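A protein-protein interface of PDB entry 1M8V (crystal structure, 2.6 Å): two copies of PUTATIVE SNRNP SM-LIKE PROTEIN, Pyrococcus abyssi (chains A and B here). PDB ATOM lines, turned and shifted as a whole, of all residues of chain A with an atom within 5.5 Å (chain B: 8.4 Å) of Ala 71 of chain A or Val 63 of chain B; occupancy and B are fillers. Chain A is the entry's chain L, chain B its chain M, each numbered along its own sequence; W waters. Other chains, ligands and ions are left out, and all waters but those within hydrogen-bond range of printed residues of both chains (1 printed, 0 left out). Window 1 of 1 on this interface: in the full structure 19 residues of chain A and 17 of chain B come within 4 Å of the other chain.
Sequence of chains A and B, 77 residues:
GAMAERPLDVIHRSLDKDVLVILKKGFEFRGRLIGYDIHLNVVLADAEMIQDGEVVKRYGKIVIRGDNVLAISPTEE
The backbone carbonyl oxygen of Leu 70 of chain A sits at hydrogen-bond distance from the backbone NH of Arg 65 of chain B, at 2.9 Å. The side-chain amide nitrogen (ND2) of Asn 68 of chain B sits at hydrogen-bond distance from the backbone carbonyl oxygen (O) of Val 69 of chain A (2.9 Å). N of Ile 72 of chain A lies within hydrogen-bond range of O of Val 63 of chain B. O of Lys 61 of chain B is in hydrogen-bond range of OG of Ser 73 of chain A, 2.8 Å away. The backbone carbonyl oxygen of Leu 70 of chain A is in hydrogen-bond range of the side-chain amide nitrogen of Asn 68 of chain B, 2.9 Å away.
The backbone carbonyl oxygen (O) of Gly 35 of chain B is in hydrogen-bond range of the backbone NH (N) of Val 43 of chain B, at 3.0 Å. The backbone carbonyl oxygen (O) of Ser 73 of chain A sits at hydrogen-bond distance from the backbone NH (N) of Leu 20 of chain A, at 2.7 Å. The backbone carbonyl oxygen (O) of Arg 65 of chain B lies within hydrogen-bond range of the side-chain amide nitrogen (ND2) of Asn 68 of chain B (3.0 Å). The side-chain amide oxygen (OD1) of Asn 41 of chain B sits at hydrogen-bond distance from the backbone NH (N) of Gly 66 of chain B (2.9 Å). The backbone carbonyl oxygen (O) of Ala 47 of chain B sits at hydrogen-bond distance from the backbone NH (N) of Tyr 59 of chain B (2.7 Å). O of Ile 22 of chain A is in hydrogen-bond range of N of Leu 70 of chain A.
Tyr 36 of chain B touches Pro 7 of chain A. OD2 of Asp 37 of chain B touches CB of Pro 7 of chain A (3.8 Å). CG of Pro 7 of chain A touches CB of Asn 41 of chain B (3.7 Å). O of Pro 7 of chain A touches CG2 of Val 63 of chain B, at 3.9 Å. CG1 of Val 10 of chain A touches CD of Lys 61 of chain B, 3.9 Å away. Tyr 59 of chain B touches Leu 20 of chain A. Ile 22 of chain A touches Tyr 59 of chain B. CD of Arg 65 of chain B touches O of Val 69 of chain A, at 3.4 Å. Ile 62 of chain B touches Ile 72 of chain A (CG1 to O, 3.6 Å). Ser 73 of chain A touches Tyr 59 of chain B.
Of the printed residues of chain B, Ala 71 of chain A touches Ile 62 (3.4 Å) and Val 63 (3.1 Å). Val 63 of chain B touches four residues of chain A. Printed residues of chain A within 4 Å of Ile 64 of chain B: Leu 70. Printed residues of chain A within 4 Å of Asp 37 of chain B: Pro 7. Leu 40 of chain B touches none of the printed residues of chain A. The nearest residue of chain A that does not touch Val 63 of chain B is Leu 70 of chain A (4.3 Å).
Of the 24 printed residues of chain B, 13 touch a printed residue of chain A. Printed residues of chain B that touch a printed residue of chain A: Leu 23, Phe 27, Tyr 36, Asp 37, Asn 41, Val 43, Tyr 59, Lys 61, Ile 62, Val 63, Ile 64, Arg 65 and Asn 68. Hydrophobic or aromatic side chains of chain A that line the printed part of chain B: Pro 7, Val 10, Leu 20, Ile 22, Leu 70, Ala 71 and Pro 74. Along chain A the printed residues that touch a printed residue of chain B span positions 7 to 74. Among the printed residues, 24 pairs touch across the chains. Among the printed residues, no Asp or Glu carboxylate lies within 4 Å of a Lys or Arg side-chain nitrogen of the other chain.
Position printed for both chains: 23.
Water W1 lies within hydrogen-bond range of O of Pro 74 of chain A (2.5 Å), O of Lys 61 of chain B (3.4 Å) and OG of Ser 73 of chain A (3.5 Å).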
ATOM      1  N   PRO A   7      24.028   6.182 -19.067  1.00  0.00           N
ATOM      2  CA  PRO A   7      24.733   5.486 -17.991  1.00  0.00           C
ATOM      3  C   PRO A   7      24.369   6.010 -16.614  1.00  0.00           C
ATOM      4  O   PRO A   7      23.957   5.238 -15.736  1.00  0.00           O
ATOM      5  CB  PRO A   7      26.187   5.729 -18.342  1.00  0.00           C
ATOM      6  CG  PRO A   7      26.161   5.577 -19.830  1.00  0.00           C
ATOM      7  CD  PRO A   7      24.904   6.330 -20.243  1.00  0.00           C
ATOM      8  N   VAL A  10      20.508   5.621 -15.595  1.00  0.00           N
ATOM      9  CA  VAL A  10      20.237   4.275 -15.105  1.00  0.00           C
ATOM     10  C   VAL A  10      20.732   4.065 -13.687  1.00  0.00           C
ATOM     11  O   VAL A  10      20.018   3.518 -12.850  1.00  0.00           O
ATOM     12  CB  VAL A  10      20.889   3.226 -16.005  1.00  0.00           C
ATOM     13  CG1 VAL A  10      20.651   1.838 -15.438  1.00  0.00           C
ATOM     14  CG2 VAL A  10      20.329   3.342 -17.418  1.00  0.00           C
ATOM     15  N   ILE A  11      21.956   4.504 -13.413  1.00  0.00           N
ATOM     16  CA  ILE A  11      22.521   4.336 -12.085  1.00  0.00           C
ATOM     17  C   ILE A  11      21.718   5.121 -11.046  1.00  0.00           C
ATOM     18  O   ILE A  11      21.345   4.584  -9.995  1.00  0.00           O
ATOM     19  CB  ILE A  11      24.003   4.778 -12.058  1.00  0.00           C
ATOM     20  CG1 ILE A  11      24.830   3.832 -12.935  1.00  0.00           C
ATOM     21  CG2 ILE A  11      24.532   4.788 -10.623  1.00  0.00           C
ATOM     22  CD1 ILE A  11      26.318   4.171 -13.017  1.00  0.00           C
ATOM     23  N   LEU A  20      23.941  -5.363  -9.325  1.00  0.00           N
ATOM     24  CA  LEU A  20      25.054  -6.290  -9.433  1.00  0.00           C
ATOM     25  C   LEU A  20      26.249  -5.500  -9.906  1.00  0.00           C
ATOM     26  O   LEU A  20      26.170  -4.805 -10.919  1.00  0.00           O
ATOM     27  CB  LEU A  20      24.740  -7.376 -10.457  1.00  0.00           C
ATOM     28  CG  LEU A  20      25.885  -8.349 -10.720  1.00  0.00           C
ATOM     29  CD1 LEU A  20      26.136  -9.201  -9.478  1.00  0.00           C
ATOM     30  CD2 LEU A  20      25.534  -9.214 -11.908  1.00  0.00           C
ATOM     31  N   VAL A  21      27.357  -5.591  -9.182  1.00  0.00           N
ATOM     32  CA  VAL A  21      28.549  -4.861  -9.586  1.00  0.00           C
ATOM     33  C   VAL A  21      29.624  -5.834 -10.039  1.00  0.00           C
ATOM     34  O   VAL A  21      30.303  -6.468  -9.233  1.00  0.00           O
ATOM     35  CB  VAL A  21      29.094  -3.969  -8.450  1.00  0.00           C
ATOM     36  CG1 VAL A  21      30.321  -3.209  -8.936  1.00  0.00           C
ATOM     37  CG2 VAL A  21      28.015  -2.975  -8.003  1.00  0.00           C
ATOM     38  N   ILE A  22      29.756  -5.954 -11.354  1.00  0.00           N
ATOM     39  CA  ILE A  22      30.733  -6.838 -11.950  1.00  0.00           C
ATOM     40  C   ILE A  22      32.059  -6.115 -12.007  1.00  0.00           C
ATOM     41  O   ILE A  22      32.194  -5.112 -12.702  1.00  0.00           O
ATOM     42  CB  ILE A  22      30.325  -7.223 -13.380  1.00  0.00           C
ATOM     43  CG1 ILE A  22      28.954  -7.890 -13.367  1.00  0.00           C
ATOM     44  CG2 ILE A  22      31.374  -8.135 -13.995  1.00  0.00           C
ATOM     45  CD1 ILE A  22      28.390  -8.116 -14.760  1.00  0.00           C
ATOM     46  N   LEU A  23      33.035  -6.631 -11.269  1.00  0.00           N
ATOM     47  CA  LEU A  23      34.371  -6.052 -11.227  1.00  0.00           C
ATOM     48  C   LEU A  23      35.222  -6.633 -12.336  1.00  0.00           C
ATOM     49  O   LEU A  23      34.892  -7.674 -12.902  1.00  0.00           O
ATOM     50  CB  LEU A  23      35.027  -6.366  -9.893  1.00  0.00           C
ATOM     51  CG  LEU A  23      34.240  -5.894  -8.683  1.00  0.00           C
ATOM     52  CD1 LEU A  23      34.846  -6.477  -7.420  1.00  0.00           C
ATOM     53  CD2 LEU A  23      34.235  -4.374  -8.651  1.00  0.00           C
ATOM     54  N   VAL A  69      35.399  -1.282 -11.702  1.00  0.00           N
ATOM     55  CA  VAL A  69      34.145  -1.777 -12.242  1.00  0.00           C
ATOM     56  C   VAL A  69      34.149  -2.124 -13.716  1.00  0.00           C
ATOM     57  O   VAL A  69      34.735  -1.440 -14.544  1.00  0.00           O
ATOM     58  CB  VAL A  69      32.993  -0.777 -11.975  1.00  0.00           C
ATOM     59  CG1 VAL A  69      31.687  -1.313 -12.548  1.00  0.00           C
ATOM     60  CG2 VAL A  69      32.842  -0.540 -10.474  1.00  0.00           C
ATOM     61  N   LEU A  70      33.488  -3.221 -14.029  1.00  0.00           N
ATOM     62  CA  LEU A  70      33.380  -3.652 -15.397  1.00  0.00           C
ATOM     63  C   LEU A  70      32.009  -3.185 -15.841  1.00  0.00           C
ATOM     64  O   LEU A  70      31.863  -2.496 -16.850  1.00  0.00           O
ATOM     65  CB  LEU A  70      33.431  -5.173 -15.494  1.00  0.00           C
ATOM     66  CG  LEU A  70      33.459  -5.643 -16.945  1.00  0.00           C
ATOM     67  CD1 LEU A  70      34.908  -5.931 -17.302  1.00  0.00           C
ATOM     68  CD2 LEU A  70      32.587  -6.869 -17.140  1.00  0.00           C
ATOM     69  N   ALA A  71      31.004  -3.572 -15.064  1.00  0.00           N
ATOM     70  CA  ALA A  71      29.643  -3.208 -15.369  1.00  0.00           C
ATOM     71  C   ALA A  71      28.786  -3.240 -14.115  1.00  0.00           C
ATOM     72  O   ALA A  71      29.138  -3.891 -13.133  1.00  0.00           O
ATOM     73  CB  ALA A  71      29.080  -4.159 -16.417  1.00  0.00           C
ATOM     74  N   ILE A  72      27.669  -2.516 -14.157  1.00  0.00           N
ATOM     75  CA  ILE A  72      26.722  -2.466 -13.057  1.00  0.00           C
ATOM     76  C   ILE A  72      25.363  -2.840 -13.646  1.00  0.00           C
ATOM     77  O   ILE A  72      25.016  -2.390 -14.736  1.00  0.00           O
ATOM     78  CB  ILE A  72      26.649  -1.060 -12.445  1.00  0.00           C
ATOM     79  CG1 ILE A  72      28.009  -0.690 -11.849  1.00  0.00           C
ATOM     80  CG2 ILE A  72      25.543  -1.007 -11.409  1.00  0.00           C
ATOM     81  CD1 ILE A  72      28.132   0.730 -11.370  1.00  0.00           C
ATOM     82  N   SER A  73      24.604  -3.672 -12.937  1.00  0.00           N
ATOM     83  CA  SER A  73      23.308  -4.098 -13.436  1.00  0.00           C
ATOM     84  C   SER A  73      22.205  -4.011 -12.393  1.00  0.00           C
ATOM     85  O   SER A  73      22.312  -4.578 -11.310  1.00  0.00           O
ATOM     86  CB  SER A  73      23.394  -5.526 -13.967  1.00  0.00           C
ATOM     87  OG  SER A  73      22.194  -5.900 -14.616  1.00  0.00           O
ATOM     88  N   PRO A  74      21.126  -3.278 -12.714  1.00  0.00           N
ATOM     89  CA  PRO A  74      19.971  -3.087 -11.837  1.00  0.00           C
ATOM     90  C   PRO A  74      19.224  -4.400 -11.644  1.00  0.00           C
ATOM     91  O   PRO A  74      19.170  -5.218 -12.555  1.00  0.00           O
ATOM     92  CB  PRO A  74      19.129  -2.075 -12.600  1.00  0.00           C
ATOM     93  CG  PRO A  74      20.132  -1.331 -13.407  1.00  0.00           C
ATOM     94  CD  PRO A  74      20.999  -2.433 -13.914  1.00  0.00           C
ATOM     95  N   LEU B  23      34.749  -6.584 -25.092  1.00  0.00           N
ATOM     96  CA  LEU B  23      35.555  -6.167 -23.952  1.00  0.00           C
ATOM     97  C   LEU B  23      37.026  -6.583 -24.062  1.00  0.00           C
ATOM     98  O   LEU B  23      37.354  -7.593 -24.687  1.00  0.00           O
ATOM     99  CB  LEU B  23      34.964  -6.728 -22.663  1.00  0.00           C
ATOM    100  CG  LEU B  23      33.629  -6.154 -22.199  1.00  0.00           C
ATOM    101  CD1 LEU B  23      33.184  -6.889 -20.942  1.00  0.00           C
ATOM    102  CD2 LEU B  23      33.769  -4.658 -21.920  1.00  0.00           C
ATOM    103  N   PHE B  27      35.692 -11.439 -23.386  1.00  0.00           N
ATOM    104  CA  PHE B  27      34.309 -11.714 -23.723  1.00  0.00           C
ATOM    105  C   PHE B  27      33.598 -10.470 -24.234  1.00  0.00           C
ATOM    106  O   PHE B  27      34.203  -9.406 -24.353  1.00  0.00           O
ATOM    107  CB  PHE B  27      33.575 -12.318 -22.527  1.00  0.00           C
ATOM    108  CG  PHE B  27      33.648 -11.497 -21.289  1.00  0.00           C
ATOM    109  CD1 PHE B  27      32.603 -10.656 -20.937  1.00  0.00           C
ATOM    110  CD2 PHE B  27      34.757 -11.577 -20.461  1.00  0.00           C
ATOM    111  CE1 PHE B  27      32.658  -9.903 -19.765  1.00  0.00           C
ATOM    112  CE2 PHE B  27      34.826 -10.830 -19.288  1.00  0.00           C
ATOM    113  CZ  PHE B  27      33.772  -9.990 -18.938  1.00  0.00           C
ATOM    114  N   PHE B  29      29.409  -8.425 -24.858  1.00  0.00           N
ATOM    115  CA  PHE B  29      27.998  -8.348 -24.538  1.00  0.00           C
ATOM    116  C   PHE B  29      27.292  -8.060 -25.834  1.00  0.00           C
ATOM    117  O   PHE B  29      27.866  -7.475 -26.748  1.00  0.00           O
ATOM    118  CB  PHE B  29      27.715  -7.234 -23.543  1.00  0.00           C
ATOM    119  CG  PHE B  29      28.207  -7.523 -22.163  1.00  0.00           C
ATOM    120  CD1 PHE B  29      29.415  -7.011 -21.721  1.00  0.00           C
ATOM    121  CD2 PHE B  29      27.461  -8.320 -21.306  1.00  0.00           C
ATOM    122  CE1 PHE B  29      29.873  -7.287 -20.443  1.00  0.00           C
ATOM    123  CE2 PHE B  29      27.910  -8.601 -20.032  1.00  0.00           C
ATOM    124  CZ  PHE B  29      29.117  -8.085 -19.597  1.00  0.00           C
ATOM    125  N   ILE B  34      20.818   1.573 -25.525  1.00  0.00           N
ATOM    126  CA  ILE B  34      19.786   2.506 -25.122  1.00  0.00           C
ATOM    127  C   ILE B  34      20.326   3.812 -24.536  1.00  0.00           C
ATOM    128  O   ILE B  34      19.546   4.673 -24.130  1.00  0.00           O
ATOM    129  CB  ILE B  34      18.837   1.857 -24.107  1.00  0.00           C
ATOM    130  CG1 ILE B  34      19.609   1.409 -22.863  1.00  0.00           C
ATOM    131  CG2 ILE B  34      18.129   0.684 -24.759  1.00  0.00           C
ATOM    132  CD1 ILE B  34      18.726   0.732 -21.812  1.00  0.00           C
ATOM    133  N   GLY B  35      21.652   3.956 -24.505  1.00  0.00           N
ATOM    134  CA  GLY B  35      22.261   5.157 -23.963  1.00  0.00           C
ATOM    135  C   GLY B  35      23.774   5.061 -23.909  1.00  0.00           C
ATOM    136  O   GLY B  35      24.338   3.988 -24.133  1.00  0.00           O
ATOM    137  N   TYR B  36      24.429   6.180 -23.605  1.00  0.00           N
ATOM    138  CA  TYR B  36      25.886   6.239 -23.518  1.00  0.00           C
ATOM    139  C   TYR B  36      26.303   7.615 -23.018  1.00  0.00           C
ATOM    140  O   TYR B  36      25.469   8.413 -22.597  1.00  0.00           O
ATOM    141  CB  TYR B  36      26.501   6.020 -24.899  1.00  0.00           C
ATOM    142  CG  TYR B  36      26.223   7.153 -25.863  1.00  0.00           C
ATOM    143  CD1 TYR B  36      27.079   8.245 -25.953  1.00  0.00           C
ATOM    144  CD2 TYR B  36      25.054   7.167 -26.625  1.00  0.00           C
ATOM    145  CE1 TYR B  36      26.773   9.327 -26.778  1.00  0.00           C
ATOM    146  CE2 TYR B  36      24.738   8.239 -27.445  1.00  0.00           C
ATOM    147  CZ  TYR B  36      25.599   9.317 -27.520  1.00  0.00           C
ATOM    148  OH  TYR B  36      25.281  10.381 -28.344  1.00  0.00           O
ATOM    149  N   ASP B  37      27.602   7.876 -23.049  1.00  0.00           N
ATOM    150  CA  ASP B  37      28.132   9.173 -22.653  1.00  0.00           C
ATOM    151  C   ASP B  37      29.462   9.410 -23.348  1.00  0.00           C
ATOM    152  O   ASP B  37      29.807   8.684 -24.280  1.00  0.00           O
ATOM    153  CB  ASP B  37      28.277   9.318 -21.128  1.00  0.00           C
ATOM    154  CG  ASP B  37      29.304   8.384 -20.524  1.00  0.00           C
ATOM    155  OD1 ASP B  37      30.327   8.096 -21.176  1.00  0.00           O
ATOM    156  OD2 ASP B  37      29.088   7.962 -19.366  1.00  0.00           O
ATOM    157  N   LEU B  40      32.467   6.771 -23.208  1.00  0.00           N
ATOM    158  CA  LEU B  40      32.163   5.587 -23.994  1.00  0.00           C
ATOM    159  C   LEU B  40      31.455   4.520 -23.174  1.00  0.00           C
ATOM    160  O   LEU B  40      31.342   3.380 -23.612  1.00  0.00           O
ATOM    161  CB  LEU B  40      33.414   5.010 -24.660  1.00  0.00           C
ATOM    162  CG  LEU B  40      33.764   5.656 -26.004  1.00  0.00           C
ATOM    163  CD1 LEU B  40      34.952   4.954 -26.620  1.00  0.00           C
ATOM    164  CD2 LEU B  40      32.578   5.544 -26.938  1.00  0.00           C
ATOM    165  N   ASN B  41      30.996   4.895 -21.979  1.00  0.00           N
ATOM    166  CA  ASN B  41      30.235   3.983 -21.146  1.00  0.00           C
ATOM    167  C   ASN B  41      29.028   3.714 -22.024  1.00  0.00           C
ATOM    168  O   ASN B  41      28.659   4.559 -22.833  1.00  0.00           O
ATOM    169  CB  ASN B  41      29.721   4.659 -19.877  1.00  0.00           C
ATOM    170  CG  ASN B  41      30.813   5.051 -18.925  1.00  0.00           C
ATOM    171  OD1 ASN B  41      31.961   4.628 -19.050  1.00  0.00           O
ATOM    172  ND2 ASN B  41      30.455   5.860 -17.941  1.00  0.00           N
ATOM    173  N   VAL B  42      28.395   2.559 -21.875  1.00  0.00           N
ATOM    174  CA  VAL B  42      27.234   2.273 -22.693  1.00  0.00           C
ATOM    175  C   VAL B  42      26.213   1.527 -21.884  1.00  0.00           C
ATOM    176  O   VAL B  42      26.558   0.838 -20.925  1.00  0.00           O
ATOM    177  CB  VAL B  42      27.595   1.426 -23.918  1.00  0.00           C
ATOM    178  CG1 VAL B  42      28.681   2.131 -24.738  1.00  0.00           C
ATOM    179  CG2 VAL B  42      28.045   0.044 -23.474  1.00  0.00           C
ATOM    180  N   VAL B  43      24.953   1.687 -22.270  1.00  0.00           N
ATOM    181  CA  VAL B  43      23.851   1.012 -21.603  1.00  0.00           C
ATOM    182  C   VAL B  43      23.175   0.135 -22.631  1.00  0.00           C
ATOM    183  O   VAL B  43      22.819   0.596 -23.712  1.00  0.00           O
ATOM    184  CB  VAL B  43      22.809   2.002 -21.046  1.00  0.00           C
ATOM    185  CG1 VAL B  43      21.732   1.231 -20.263  1.00  0.00           C
ATOM    186  CG2 VAL B  43      23.506   3.052 -20.162  1.00  0.00           C
ATOM    187  N   LEU B  44      23.010  -1.139 -22.299  1.00  0.00           N
ATOM    188  CA  LEU B  44      22.373  -2.075 -23.208  1.00  0.00           C
ATOM    189  C   LEU B  44      21.172  -2.665 -22.520  1.00  0.00           C
ATOM    190  O   LEU B  44      21.134  -2.786 -21.294  1.00  0.00           O
ATOM    191  CB  LEU B  44      23.332  -3.203 -23.590  1.00  0.00           C
ATOM    192  CG  LEU B  44      24.684  -2.823 -24.186  1.00  0.00           C
ATOM    193  CD1 LEU B  44      25.552  -4.076 -24.269  1.00  0.00           C
ATOM    194  CD2 LEU B  44      24.501  -2.201 -25.558  1.00  0.00           C
ATOM    195  N   ALA B  45      20.189  -3.024 -23.330  1.00  0.00           N
ATOM    196  CA  ALA B  45      18.967  -3.629 -22.844  1.00  0.00           C
ATOM    197  C   ALA B  45      18.933  -5.044 -23.400  1.00  0.00           C
ATOM    198  O   ALA B  45      19.533  -5.315 -24.448  1.00  0.00           O
ATOM    199  CB  ALA B  45      17.759  -2.846 -23.351  1.00  0.00           C
ATOM    200  N   ALA B  47      20.452  -7.655 -22.793  1.00  0.00           N
ATOM    201  CA  ALA B  47      21.812  -8.009 -23.140  1.00  0.00           C
ATOM    202  C   ALA B  47      22.178  -9.427 -22.704  1.00  0.00           C
ATOM    203  O   ALA B  47      21.691  -9.941 -21.694  1.00  0.00           O
ATOM    204  CB  ALA B  47      22.780  -6.987 -22.521  1.00  0.00           C
ATOM    205  N   MET B  49      25.617 -11.807 -22.116  1.00  0.00           N
ATOM    206  CA  MET B  49      27.077 -11.906 -22.024  1.00  0.00           C
ATOM    207  C   MET B  49      27.539 -13.134 -22.818  1.00  0.00           C
ATOM    208  O   MET B  49      27.017 -14.231 -22.640  1.00  0.00           O
ATOM    209  CB  MET B  49      27.510 -12.045 -20.563  1.00  0.00           C
ATOM    210  CG  MET B  49      29.010 -12.227 -20.364  1.00  0.00           C
ATOM    211  SD  MET B  49      29.456 -12.518 -18.622  1.00  0.00           S
ATOM    212  CE  MET B  49      30.095 -10.928 -18.126  1.00  0.00           C
ATOM    213  N   TYR B  59      21.110  -9.969 -19.041  1.00  0.00           N
ATOM    214  CA  TYR B  59      20.779  -8.792 -18.240  1.00  0.00           C
ATOM    215  C   TYR B  59      19.737  -7.934 -18.958  1.00  0.00           C
ATOM    216  O   TYR B  59      19.960  -7.473 -20.084  1.00  0.00           O
ATOM    217  CB  TYR B  59      22.021  -7.937 -17.973  1.00  0.00           C
ATOM    218  CG  TYR B  59      23.250  -8.697 -17.521  1.00  0.00           C
ATOM    219  CD1 TYR B  59      24.226  -9.087 -18.435  1.00  0.00           C
ATOM    220  CD2 TYR B  59      23.449  -9.002 -16.176  1.00  0.00           C
ATOM    221  CE1 TYR B  59      25.366  -9.750 -18.023  1.00  0.00           C
ATOM    222  CE2 TYR B  59      24.583  -9.670 -15.758  1.00  0.00           C
ATOM    223  CZ  TYR B  59      25.538 -10.039 -16.685  1.00  0.00           C
ATOM    224  OH  TYR B  59      26.664 -10.705 -16.267  1.00  0.00           O
ATOM    225  N   GLY B  60      18.596  -7.729 -18.303  1.00  0.00           N
ATOM    226  CA  GLY B  60      17.546  -6.914 -18.885  1.00  0.00           C
ATOM    227  C   GLY B  60      18.098  -5.532 -19.167  1.00  0.00           C
ATOM    228  O   GLY B  60      17.681  -4.864 -20.115  1.00  0.00           O
ATOM    229  N   LYS B  61      19.055  -5.113 -18.339  1.00  0.00           N
ATOM    230  CA  LYS B  61      19.684  -3.809 -18.487  1.00  0.00           C
ATOM    231  C   LYS B  61      21.060  -3.792 -17.810  1.00  0.00           C
ATOM    232  O   LYS B  61      21.225  -4.297 -16.701  1.00  0.00           O
ATOM    233  CB  LYS B  61      18.776  -2.725 -17.884  1.00  0.00           C
ATOM    234  CG  LYS B  61      19.233  -1.306 -18.163  1.00  0.00           C
ATOM    235  CD  LYS B  61      18.213  -0.280 -17.670  1.00  0.00           C
ATOM    236  CE  LYS B  61      16.934  -0.307 -18.501  1.00  0.00           C
ATOM    237  NZ  LYS B  61      15.902   0.641 -17.986  1.00  0.00           N
ATOM    238  N   ILE B  62      22.045  -3.203 -18.478  1.00  0.00           N
ATOM    239  CA  ILE B  62      23.386  -3.148 -17.922  1.00  0.00           C
ATOM    240  C   ILE B  62      24.207  -1.944 -18.375  1.00  0.00           C
ATOM    241  O   ILE B  62      24.209  -1.583 -19.553  1.00  0.00           O
ATOM    242  CB  ILE B  62      24.191  -4.441 -18.271  1.00  0.00           C
ATOM    243  CG1 ILE B  62      25.574  -4.404 -17.611  1.00  0.00           C
ATOM    244  CG2 ILE B  62      24.378  -4.566 -19.787  1.00  0.00           C
ATOM    245  CD1 ILE B  62      26.323  -5.727 -17.700  1.00  0.00           C
ATOM    246  N   VAL B  63      24.905  -1.334 -17.422  1.00  0.00           N
ATOM    247  CA  VAL B  63      25.783  -0.201 -17.692  1.00  0.00           C
ATOM    248  C   VAL B  63      27.242  -0.726 -17.687  1.00  0.00           C
ATOM    249  O   VAL B  63      27.739  -1.191 -16.665  1.00  0.00           O
ATOM    250  CB  VAL B  63      25.641   0.905 -16.600  1.00  0.00           C
ATOM    251  CG1 VAL B  63      26.599   2.062 -16.896  1.00  0.00           C
ATOM    252  CG2 VAL B  63      24.201   1.391 -16.517  1.00  0.00           C
ATOM    253  N   ILE B  64      27.910  -0.647 -18.833  1.00  0.00           N
ATOM    254  CA  ILE B  64      29.294  -1.092 -18.988  1.00  0.00           C
ATOM    255  C   ILE B  64      30.227   0.109 -18.928  1.00  0.00           C
ATOM    256  O   ILE B  64      29.978   1.117 -19.586  1.00  0.00           O
ATOM    257  CB  ILE B  64      29.495  -1.758 -20.373  1.00  0.00           C
ATOM    258  CG1 ILE B  64      28.547  -2.944 -20.530  1.00  0.00           C
ATOM    259  CG2 ILE B  64      30.951  -2.150 -20.566  1.00  0.00           C
ATOM    260  CD1 ILE B  64      28.444  -3.446 -21.953  1.00  0.00           C
ATOM    261  N   ARG B  65      31.310   0.010 -18.167  1.00  0.00           N
ATOM    262  CA  ARG B  65      32.266   1.116 -18.069  1.00  0.00           C
ATOM    263  C   ARG B  65      33.142   1.122 -19.331  1.00  0.00           C
ATOM    264  O   ARG B  65      33.940   0.214 -19.547  1.00  0.00           O
ATOM    265  CB  ARG B  65      33.120   0.942 -16.815  1.00  0.00           C
ATOM    266  CG  ARG B  65      33.885   2.173 -16.362  1.00  0.00           C
ATOM    267  CD  ARG B  65      34.613   1.905 -15.043  1.00  0.00           C
ATOM    268  NE  ARG B  65      34.868   3.143 -14.311  1.00  0.00           N
ATOM    269  CZ  ARG B  65      35.950   3.906 -14.447  1.00  0.00           C
ATOM    270  NH1 ARG B  65      36.917   3.562 -15.291  1.00  0.00           N
ATOM    271  NH2 ARG B  65      36.050   5.032 -13.747  1.00  0.00           N
ATOM    272  N   GLY B  66      32.973   2.143 -20.170  1.00  0.00           N
ATOM    273  CA  GLY B  66      33.730   2.249 -21.415  1.00  0.00           C
ATOM    274  C   GLY B  66      35.214   1.974 -21.298  1.00  0.00           C
ATOM    275  O   GLY B  66      35.893   1.708 -22.279  1.00  0.00           O
ATOM    276  N   ASN B  68      36.445  -0.473 -20.112  1.00  0.00           N
ATOM    277  CA  ASN B  68      36.589  -1.894 -20.361  1.00  0.00           C
ATOM    278  C   ASN B  68      36.306  -2.281 -21.797  1.00  0.00           C
ATOM    279  O   ASN B  68      36.498  -3.442 -22.172  1.00  0.00           O
ATOM    280  CB  ASN B  68      35.628  -2.655 -19.457  1.00  0.00           C
ATOM    281  CG  ASN B  68      35.751  -2.240 -18.011  1.00  0.00           C
ATOM    282  OD1 ASN B  68      36.823  -2.363 -17.412  1.00  0.00           O
ATOM    283  ND2 ASN B  68      34.654  -1.745 -17.436  1.00  0.00           N
HETATM  284  O   HOH W   1      18.756  -5.853 -14.908  1.00  0.00           O
